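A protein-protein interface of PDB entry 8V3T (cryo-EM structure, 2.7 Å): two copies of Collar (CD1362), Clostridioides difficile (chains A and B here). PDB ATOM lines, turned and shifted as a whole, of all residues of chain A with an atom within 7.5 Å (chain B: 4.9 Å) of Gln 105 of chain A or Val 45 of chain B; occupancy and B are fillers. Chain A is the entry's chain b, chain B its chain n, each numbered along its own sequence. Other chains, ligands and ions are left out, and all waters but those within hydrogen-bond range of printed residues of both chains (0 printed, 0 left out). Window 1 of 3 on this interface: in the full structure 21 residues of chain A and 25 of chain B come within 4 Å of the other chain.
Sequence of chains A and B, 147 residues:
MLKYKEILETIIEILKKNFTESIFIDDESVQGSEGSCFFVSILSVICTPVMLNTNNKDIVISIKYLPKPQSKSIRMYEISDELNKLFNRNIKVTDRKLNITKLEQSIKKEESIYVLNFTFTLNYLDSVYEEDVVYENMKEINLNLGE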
ATOM      1  N   MET A  76      -4.596 -10.643 -27.224  1.00  0.00           N
ATOM      2  CA  MET A  76      -4.877  -9.852 -26.032  1.00  0.00           C
ATOM      3  C   MET A  76      -4.860 -10.714 -24.781  1.00  0.00           C
ATOM      4  O   MET A  76      -4.490 -10.237 -23.703  1.00  0.00           O
ATOM      5  CB  MET A  76      -6.230  -9.152 -26.168  1.00  0.00           C
ATOM      6  CG  MET A  76      -6.338  -7.829 -25.443  1.00  0.00           C
ATOM      7  SD  MET A  76      -7.869  -6.947 -25.803  1.00  0.00           S
ATOM      8  CE  MET A  76      -9.009  -8.309 -26.031  1.00  0.00           C
ATOM      9  N   TYR A  77      -5.249 -11.982 -24.902  1.00  0.00           N
ATOM     10  CA  TYR A  77      -5.241 -12.874 -23.748  1.00  0.00           C
ATOM     11  C   TYR A  77      -3.879 -13.501 -23.470  1.00  0.00           C
ATOM     12  O   TYR A  77      -3.625 -13.903 -22.329  1.00  0.00           O
ATOM     13  CB  TYR A  77      -6.294 -13.973 -23.924  1.00  0.00           C
ATOM     14  CG  TYR A  77      -7.704 -13.468 -23.724  1.00  0.00           C
ATOM     15  CD1 TYR A  77      -8.199 -13.228 -22.450  1.00  0.00           C
ATOM     16  CD2 TYR A  77      -8.530 -13.202 -24.806  1.00  0.00           C
ATOM     17  CE1 TYR A  77      -9.480 -12.755 -22.259  1.00  0.00           C
ATOM     18  CE2 TYR A  77      -9.813 -12.729 -24.624  1.00  0.00           C
ATOM     19  CZ  TYR A  77     -10.282 -12.508 -23.348  1.00  0.00           C
ATOM     20  OH  TYR A  77     -11.559 -12.036 -23.161  1.00  0.00           O
ATOM     21  N   ILE A  79      -1.001 -11.690 -24.076  1.00  0.00           N
ATOM     22  CA  ILE A  79      -0.193 -10.561 -23.633  1.00  0.00           C
ATOM     23  C   ILE A  79      -0.407 -10.301 -22.148  1.00  0.00           C
ATOM     24  O   ILE A  79       0.520  -9.897 -21.435  1.00  0.00           O
ATOM     25  CB  ILE A  79      -0.517  -9.327 -24.493  1.00  0.00           C
ATOM     26  CG1 ILE A  79       0.222  -9.424 -25.827  1.00  0.00           C
ATOM     27  CG2 ILE A  79      -0.162  -8.040 -23.770  1.00  0.00           C
ATOM     28  CD1 ILE A  79       0.141  -8.186 -26.659  1.00  0.00           C
ATOM     29  N   SER A  80      -1.626 -10.529 -21.658  1.00  0.00           N
ATOM     30  CA  SER A  80      -1.895 -10.351 -20.236  1.00  0.00           C
ATOM     31  C   SER A  80      -1.076 -11.322 -19.395  1.00  0.00           C
ATOM     32  O   SER A  80      -0.568 -10.953 -18.331  1.00  0.00           O
ATOM     33  CB  SER A  80      -3.387 -10.522 -19.962  1.00  0.00           C
ATOM     34  OG  SER A  80      -3.707 -11.876 -19.702  1.00  0.00           O
ATOM     35  N   ASP A  81      -0.933 -12.566 -19.857  1.00  0.00           N
ATOM     36  CA  ASP A  81      -0.096 -13.531 -19.149  1.00  0.00           C
ATOM     37  C   ASP A  81       1.363 -13.092 -19.130  1.00  0.00           C
ATOM     38  O   ASP A  81       2.036 -13.174 -18.090  1.00  0.00           O
ATOM     39  CB  ASP A  81      -0.231 -14.905 -19.801  1.00  0.00           C
ATOM     40  CG  ASP A  81      -1.548 -15.574 -19.477  1.00  0.00           C
ATOM     41  OD1 ASP A  81      -2.264 -15.083 -18.581  1.00  0.00           O
ATOM     42  OD2 ASP A  81      -1.882 -16.577 -20.139  1.00  0.00           O
ATOM     43  N   LEU A  83       2.543 -10.008 -19.369  1.00  0.00           N
ATOM     44  CA  LEU A  83       2.643  -8.859 -18.476  1.00  0.00           C
ATOM     45  C   LEU A  83       2.552  -9.278 -17.018  1.00  0.00           C
ATOM     46  O   LEU A  83       3.240  -8.711 -16.163  1.00  0.00           O
ATOM     47  CB  LEU A  83       1.550  -7.842 -18.801  1.00  0.00           C
ATOM     48  CG  LEU A  83       1.771  -6.965 -20.033  1.00  0.00           C
ATOM     49  CD1 LEU A  83       0.519  -6.165 -20.342  1.00  0.00           C
ATOM     50  CD2 LEU A  83       2.963  -6.048 -19.834  1.00  0.00           C
ATOM     51  N   ASN A  84       1.711 -10.269 -16.718  1.00  0.00           N
ATOM     52  CA  ASN A  84       1.625 -10.792 -15.363  1.00  0.00           C
ATOM     53  C   ASN A  84       2.956 -11.379 -14.923  1.00  0.00           C
ATOM     54  O   ASN A  84       3.360 -11.223 -13.764  1.00  0.00           O
ATOM     55  CB  ASN A  84       0.517 -11.840 -15.279  1.00  0.00           C
ATOM     56  CG  ASN A  84      -0.171 -11.852 -13.936  1.00  0.00           C
ATOM     57  OD1 ASN A  84      -0.277 -12.893 -13.291  1.00  0.00           O
ATOM     58  ND2 ASN A  84      -0.641 -10.691 -13.503  1.00  0.00           N
ATOM     59  N   LEU A 103      -2.506  -5.178  -8.286  1.00  0.00           N
ATOM     60  CA  LEU A 103      -2.610  -5.234  -9.737  1.00  0.00           C
ATOM     61  C   LEU A 103      -4.078  -5.317 -10.122  1.00  0.00           C
ATOM     62  O   LEU A 103      -4.819  -6.137  -9.571  1.00  0.00           O
ATOM     63  CB  LEU A 103      -1.851  -6.441 -10.296  1.00  0.00           C
ATOM     64  CG  LEU A 103      -0.332  -6.476 -10.140  1.00  0.00           C
ATOM     65  CD1 LEU A 103       0.122  -7.863  -9.746  1.00  0.00           C
ATOM     66  CD2 LEU A 103       0.325  -6.074 -11.441  1.00  0.00           C
ATOM     67  N   GLU A 104      -4.496  -4.475 -11.062  1.00  0.00           N
ATOM     68  CA  GLU A 104      -5.863  -4.484 -11.559  1.00  0.00           C
ATOM     69  C   GLU A 104      -5.856  -4.511 -13.079  1.00  0.00           C
ATOM     70  O   GLU A 104      -4.986  -3.923 -13.725  1.00  0.00           O
ATOM     71  CB  GLU A 104      -6.662  -3.275 -11.065  1.00  0.00           C
ATOM     72  CG  GLU A 104      -6.797  -3.199  -9.558  1.00  0.00           C
ATOM     73  CD  GLU A 104      -7.657  -2.037  -9.114  1.00  0.00           C
ATOM     74  OE1 GLU A 104      -8.627  -1.708  -9.829  1.00  0.00           O
ATOM     75  OE2 GLU A 104      -7.364  -1.450  -8.051  1.00  0.00           O
ATOM     76  N   GLN A 105      -6.844  -5.198 -13.641  1.00  0.00           N
ATOM     77  CA  GLN A 105      -6.904  -5.435 -15.074  1.00  0.00           C
ATOM     78  C   GLN A 105      -8.358  -5.447 -15.513  1.00  0.00           C
ATOM     79  O   GLN A 105      -9.227  -5.929 -14.782  1.00  0.00           O
ATOM     80  CB  GLN A 105      -6.227  -6.761 -15.431  1.00  0.00           C
ATOM     81  CG  GLN A 105      -6.156  -7.055 -16.908  1.00  0.00           C
ATOM     82  CD  GLN A 105      -5.481  -8.375 -17.197  1.00  0.00           C
ATOM     83  OE1 GLN A 105      -5.397  -8.802 -18.345  1.00  0.00           O
ATOM     84  NE2 GLN A 105      -4.993  -9.033 -16.152  1.00  0.00           N
ATOM     85  N   SER A 106      -8.620  -4.914 -16.704  1.00  0.00           N
ATOM     86  CA  SER A 106      -9.969  -4.908 -17.244  1.00  0.00           C
ATOM     87  C   SER A 106      -9.906  -4.986 -18.760  1.00  0.00           C
ATOM     88  O   SER A 106      -8.934  -4.549 -19.380  1.00  0.00           O
ATOM     89  CB  SER A 106     -10.745  -3.659 -16.813  1.00  0.00           C
ATOM     90  OG  SER A 106     -10.224  -2.496 -17.429  1.00  0.00           O
ATOM     91  N   ILE A 107     -10.955  -5.552 -19.349  1.00  0.00           N
ATOM     92  CA  ILE A 107     -11.122  -5.610 -20.794  1.00  0.00           C
ATOM     93  C   ILE A 107     -12.466  -4.977 -21.115  1.00  0.00           C
ATOM     94  O   ILE A 107     -13.518  -5.561 -20.828  1.00  0.00           O
ATOM     95  CB  ILE A 107     -11.045  -7.042 -21.339  1.00  0.00           C
ATOM     96  CG1 ILE A 107      -9.683  -7.657 -21.015  1.00  0.00           C
ATOM     97  CG2 ILE A 107     -11.298  -7.052 -22.836  1.00  0.00           C
ATOM     98  CD1 ILE A 107      -9.515  -9.068 -21.512  1.00  0.00           C
ATOM     99  N   LEU A 116      -7.333  -3.766 -23.892  1.00  0.00           N
ATOM    100  CA  LEU A 116      -6.842  -4.304 -22.631  1.00  0.00           C
ATOM    101  C   LEU A 116      -6.180  -3.189 -21.833  1.00  0.00           C
ATOM    102  O   LEU A 116      -5.363  -2.438 -22.373  1.00  0.00           O
ATOM    103  CB  LEU A 116      -5.849  -5.442 -22.870  1.00  0.00           C
ATOM    104  CG  LEU A 116      -5.030  -5.908 -21.666  1.00  0.00           C
ATOM    105  CD1 LEU A 116      -5.923  -6.575 -20.639  1.00  0.00           C
ATOM    106  CD2 LEU A 116      -3.923  -6.848 -22.103  1.00  0.00           C
ATOM    107  N   ASN A 117      -6.534  -3.085 -20.554  1.00  0.00           N
ATOM    108  CA  ASN A 117      -6.003  -2.058 -19.664  1.00  0.00           C
ATOM    109  C   ASN A 117      -5.357  -2.743 -18.465  1.00  0.00           C
ATOM    110  O   ASN A 117      -6.057  -3.291 -17.607  1.00  0.00           O
ATOM    111  CB  ASN A 117      -7.106  -1.100 -19.222  1.00  0.00           C
ATOM    112  CG  ASN A 117      -6.565   0.211 -18.693  1.00  0.00           C
ATOM    113  OD1 ASN A 117      -5.428   0.288 -18.233  1.00  0.00           O
ATOM    114  ND2 ASN A 117      -7.382   1.254 -18.754  1.00  0.00           N
ATOM    115  N   PHE A 118      -4.029  -2.708 -18.406  1.00  0.00           N
ATOM    116  CA  PHE A 118      -3.256  -3.337 -17.341  1.00  0.00           C
ATOM    117  C   PHE A 118      -2.663  -2.243 -16.462  1.00  0.00           C
ATOM    118  O   PHE A 118      -1.890  -1.410 -16.944  1.00  0.00           O
ATOM    119  CB  PHE A 118      -2.160  -4.226 -17.933  1.00  0.00           C
ATOM    120  CG  PHE A 118      -1.382  -5.008 -16.913  1.00  0.00           C
ATOM    121  CD1 PHE A 118      -0.296  -4.446 -16.263  1.00  0.00           C
ATOM    122  CD2 PHE A 118      -1.726  -6.315 -16.615  1.00  0.00           C
ATOM    123  CE1 PHE A 118       0.421  -5.167 -15.331  1.00  0.00           C
ATOM    124  CE2 PHE A 118      -1.011  -7.040 -15.684  1.00  0.00           C
ATOM    125  CZ  PHE A 118       0.063  -6.465 -15.041  1.00  0.00           C
ATOM    126  N   THR A 119      -3.025  -2.245 -15.178  1.00  0.00           N
ATOM    127  CA  THR A 119      -2.589  -1.217 -14.243  1.00  0.00           C
ATOM    128  C   THR A 119      -2.052  -1.850 -12.967  1.00  0.00           C
ATOM    129  O   THR A 119      -2.484  -2.931 -12.560  1.00  0.00           O
ATOM    130  CB  THR A 119      -3.728  -0.246 -13.872  1.00  0.00           C
ATOM    131  OG1 THR A 119      -4.489  -0.792 -12.789  1.00  0.00           O
ATOM    132  CG2 THR A 119      -4.648   0.007 -15.054  1.00  0.00           C
ATOM    133  N   PHE A 120      -1.103  -1.159 -12.338  1.00  0.00           N
ATOM    134  CA  PHE A 120      -0.585  -1.559 -11.037  1.00  0.00           C
ATOM    135  C   PHE A 120      -0.133  -0.315 -10.285  1.00  0.00           C
ATOM    136  O   PHE A 120       0.112   0.737 -10.880  1.00  0.00           O
ATOM    137  CB  PHE A 120       0.562  -2.571 -11.159  1.00  0.00           C
ATOM    138  CG  PHE A 120       1.749  -2.069 -11.933  1.00  0.00           C
ATOM    139  CD1 PHE A 120       1.784  -2.157 -13.313  1.00  0.00           C
ATOM    140  CD2 PHE A 120       2.840  -1.530 -11.275  1.00  0.00           C
ATOM    141  CE1 PHE A 120       2.875  -1.704 -14.022  1.00  0.00           C
ATOM    142  CE2 PHE A 120       3.935  -1.075 -11.979  1.00  0.00           C
ATOM    143  CZ  PHE A 120       3.953  -1.162 -13.354  1.00  0.00           C
ATOM    144  N   TYR B   4      -4.659 -17.366 -18.143  1.00  0.00           N
ATOM    145  CA  TYR B   4      -6.018 -16.905 -18.415  1.00  0.00           C
ATOM    146  C   TYR B   4      -6.557 -17.508 -19.707  1.00  0.00           C
ATOM    147  O   TYR B   4      -7.756 -17.807 -19.814  1.00  0.00           O
ATOM    148  CB  TYR B   4      -6.045 -15.380 -18.487  1.00  0.00           C
ATOM    149  CG  TYR B   4      -5.559 -14.696 -17.230  1.00  0.00           C
ATOM    150  CD1 TYR B   4      -5.914 -15.166 -15.973  1.00  0.00           C
ATOM    151  CD2 TYR B   4      -4.746 -13.574 -17.301  1.00  0.00           C
ATOM    152  CE1 TYR B   4      -5.468 -14.540 -14.825  1.00  0.00           C
ATOM    153  CE2 TYR B   4      -4.296 -12.943 -16.161  1.00  0.00           C
ATOM    154  CZ  TYR B   4      -4.659 -13.428 -14.927  1.00  0.00           C
ATOM    155  OH  TYR B   4      -4.210 -12.797 -13.791  1.00  0.00           O
ATOM    156  N   ILE B  42     -13.213 -11.919 -20.439  1.00  0.00           N
ATOM    157  CA  ILE B  42     -12.848 -11.767 -19.036  1.00  0.00           C
ATOM    158  C   ILE B  42     -12.978 -10.293 -18.679  1.00  0.00           C
ATOM    159  O   ILE B  42     -12.329  -9.439 -19.290  1.00  0.00           O
ATOM    160  CB  ILE B  42     -11.425 -12.280 -18.767  1.00  0.00           C
ATOM    161  CG1 ILE B  42     -11.337 -13.781 -19.050  1.00  0.00           C
ATOM    162  CG2 ILE B  42     -11.014 -11.979 -17.336  1.00  0.00           C
ATOM    163  CD1 ILE B  42     -10.085 -14.433 -18.511  1.00  0.00           C
ATOM    164  N   LEU B  43     -13.816  -9.992 -17.687  1.00  0.00           N
ATOM    165  CA  LEU B  43     -14.168  -8.603 -17.421  1.00  0.00           C
ATOM    166  C   LEU B  43     -13.123  -7.905 -16.559  1.00  0.00           C
ATOM    167  O   LEU B  43     -12.660  -6.812 -16.900  1.00  0.00           O
ATOM    168  CB  LEU B  43     -15.544  -8.531 -16.760  1.00  0.00           C
ATOM    169  CG  LEU B  43     -16.180  -7.144 -16.714  1.00  0.00           C
ATOM    170  CD1 LEU B  43     -16.408  -6.628 -18.123  1.00  0.00           C
ATOM    171  CD2 LEU B  43     -17.482  -7.179 -15.939  1.00  0.00           C
ATOM    172  N   SER B  44     -12.736  -8.513 -15.441  1.00  0.00           N
ATOM    173  CA  SER B  44     -11.797  -7.856 -14.543  1.00  0.00           C
ATOM    174  C   SER B  44     -11.021  -8.897 -13.753  1.00  0.00           C
ATOM    175  O   SER B  44     -11.528  -9.984 -13.463  1.00  0.00           O
ATOM    176  CB  SER B  44     -12.515  -6.897 -13.588  1.00  0.00           C
ATOM    177  OG  SER B  44     -13.499  -7.573 -12.829  1.00  0.00           O
ATOM    178  N   VAL B  45      -9.783  -8.545 -13.414  1.00  0.00           N
ATOM    179  CA  VAL B  45      -8.916  -9.353 -12.565  1.00  0.00           C
ATOM    180  C   VAL B  45      -8.322  -8.445 -11.500  1.00  0.00           C
ATOM    181  O   VAL B  45      -7.809  -7.367 -11.816  1.00  0.00           O
ATOM    182  CB  VAL B  45      -7.797 -10.042 -13.370  1.00  0.00           C
ATOM    183  CG1 VAL B  45      -6.955 -10.919 -12.460  1.00  0.00           C
ATOM    184  CG2 VAL B  45      -8.377 -10.861 -14.508  1.00  0.00           C
ATOM    185  N   ILE B  46      -8.393  -8.876 -10.244  1.00  0.00           N
ATOM    186  CA  ILE B  46      -7.833  -8.142  -9.117  1.00  0.00           C
ATOM    187  C   ILE B  46      -6.874  -9.066  -8.381  1.00  0.00           C
ATOM    188  O   ILE B  46      -7.247 -10.184  -8.008  1.00  0.00           O
ATOM    189  CB  ILE B  46      -8.932  -7.622  -8.174  1.00  0.00           C
ATOM    190  CG1 ILE B  46      -9.873  -6.680  -8.926  1.00  0.00           C
ATOM    191  CG2 ILE B  46      -8.317  -6.915  -6.980  1.00  0.00           C
ATOM    192  CD1 ILE B  46     -10.827  -5.927  -8.033  1.00  0.00           C
ATOM    193  N   CYS B  47      -5.646  -8.600  -8.174  1.00  0.00           N
ATOM    194  CA  CYS B  47      -4.577  -9.411  -7.605  1.00  0.00           C
ATOM    195  C   CYS B  47      -4.022  -8.724  -6.366  1.00  0.00           C
ATOM    196  O   CYS B  47      -3.636  -7.552  -6.422  1.00  0.00           O
ATOM    197  CB  CYS B  47      -3.472  -9.642  -8.637  1.00  0.00           C
ATOM    198  SG  CYS B  47      -2.205 -10.816  -8.138  1.00  0.00           S
ATOM    199  N   ASP B  58      -9.190 -12.512  -7.958  1.00  0.00           N
ATOM    200  CA  ASP B  58     -10.627 -12.512  -8.203  1.00  0.00           C
ATOM    201  C   ASP B  58     -10.857 -12.194  -9.673  1.00  0.00           C
ATOM    202  O   ASP B  58     -10.406 -11.152 -10.159  1.00  0.00           O
ATOM    203  CB  ASP B  58     -11.343 -11.489  -7.318  1.00  0.00           C
ATOM    204  CG  ASP B  58     -11.442 -11.933  -5.874  1.00  0.00           C
ATOM    205  OD1 ASP B  58     -12.524 -11.777  -5.273  1.00  0.00           O
ATOM    206  OD2 ASP B  58     -10.430 -12.425  -5.334  1.00  0.00           O
ATOM    207  N   ILE B  59     -11.554 -13.082 -10.374  1.00  0.00           N
ATOM    208  CA  ILE B  59     -11.775 -12.956 -11.810  1.00  0.00           C
ATOM    209  C   ILE B  59     -13.273 -12.912 -12.073  1.00  0.00           C
ATOM    210  O   ILE B  59     -14.019 -13.767 -11.584  1.00  0.00           O
ATOM    211  CB  ILE B  59     -11.120 -14.110 -12.589  1.00  0.00           C
ATOM    212  CG1 ILE B  59      -9.655 -14.262 -12.184  1.00  0.00           C
ATOM    213  CG2 ILE B  59     -11.242 -13.879 -14.083  1.00  0.00           C
ATOM    214  CD1 ILE B  59      -8.949 -15.396 -12.880  1.00  0.00           C
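The backbone NH of Gln 105 of chain A lies within hydrogen-bond range of the backbone carbonyl oxygen of Val 45 of chain B (3.0 Å).
The backbone carbonyl oxygen (O) of Leu 103 of chain A is in hydrogen-bond range of the backbone NH (N) of Cys 47 of chain B (2.9 Å).
O of Leu 43 of chain B is in hydrogen-bond range of N of Ile 107 of chain A (3.2 Å).
OH of Tyr 77 of chain A sits at hydrogen-bond distance from N of Ile 42 of chain B.
The side-chain carboxylate (OD1) of Asp 81 of chain A sits close to the backbone NH (N) of Tyr 4 of chain B, at 3.3 Å.
The backbone carbonyl oxygen (O) of Ile 46 of chain B sits at hydrogen-bond distance from the backbone NH (N) of Asp 58 of chain B (3.0 Å).
The backbone carbonyl oxygen (O) of Ser 106 of chain A lies within hydrogen-bond range of the backbone NH (N) of Asn 117 of chain A.
The backbone NH (N) of Glu 104 of chain A is in hydrogen-bond range of the backbone carbonyl oxygen (O) of Thr 119 of chain A, at 2.9 Å.
O of Tyr 77 of chain A lies within hydrogen-bond range of OG of Ser 80 of chain A.
Among the printed residues, merely in contact across the chains: Ser 80 of chain A with Tyr 4 of chain B, Gln 105 of chain A with Ser 44 of chain B, Ser 106 of chain A with Leu 43 of chain B, Ile 107 of chain A with Ile 42 of chain B, Glu 104 of chain A with Val 45 of chain B, Leu 103 of chain A with Ile 46 of chain B, Leu 103 of chain A with Val 45 of chain B, Asn 84 of chain A with Tyr 4 of chain B and Gln 105 of chain A with Tyr 4 of chain B.
Printed residues of chain B within 4 Å of Leu 103 of chain A: Val 45 (3.9 Å), Ile 46 (3.6 Å) and Cys 47 (2.9 Å).
Of the printed residues of chain B, Glu 104 of chain A touches Val 45.
Gln 105 of chain A touches just these residues of chain B: Tyr 4, Ser 44 and Val 45.
Thr 119 of chain A touches none of the printed residues of chain B.
Printed residues of chain A within 4 Å of Ile 42 of chain B: Tyr 77 and Ile 107.
Of chain A, only Leu 103 (3.9 Å), Glu 104 (3.5 Å) and Gln 105 (3.0 Å) come within 4 Å of Val 45 of chain B.
Of the printed residues of chain A, Cys 47 of chain B touches Leu 103.
Of the 9 printed residues of chain B, 7 touch a printed residue of chain A.
Hydrophobic or aromatic side chains of chain B that line the printed part of chain A: Tyr 4 and Ile 42.
Of the 17 printed residues of chain A, 9 touch a printed residue of chain B.
Hydrophobic or aromatic side chains of chain A that line the printed part of chain B: Tyr 77, Leu 103 and Ile 107.
Among the printed residues, no Asp or Glu carboxylate lies within 4 Å of a Lys or Arg side-chain nitrogen of the other chain.
No position is printed for both chains.
Of the 14 pairs that touch across the chains among the printed residues, none has its exchanged pair printed and touching as well.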
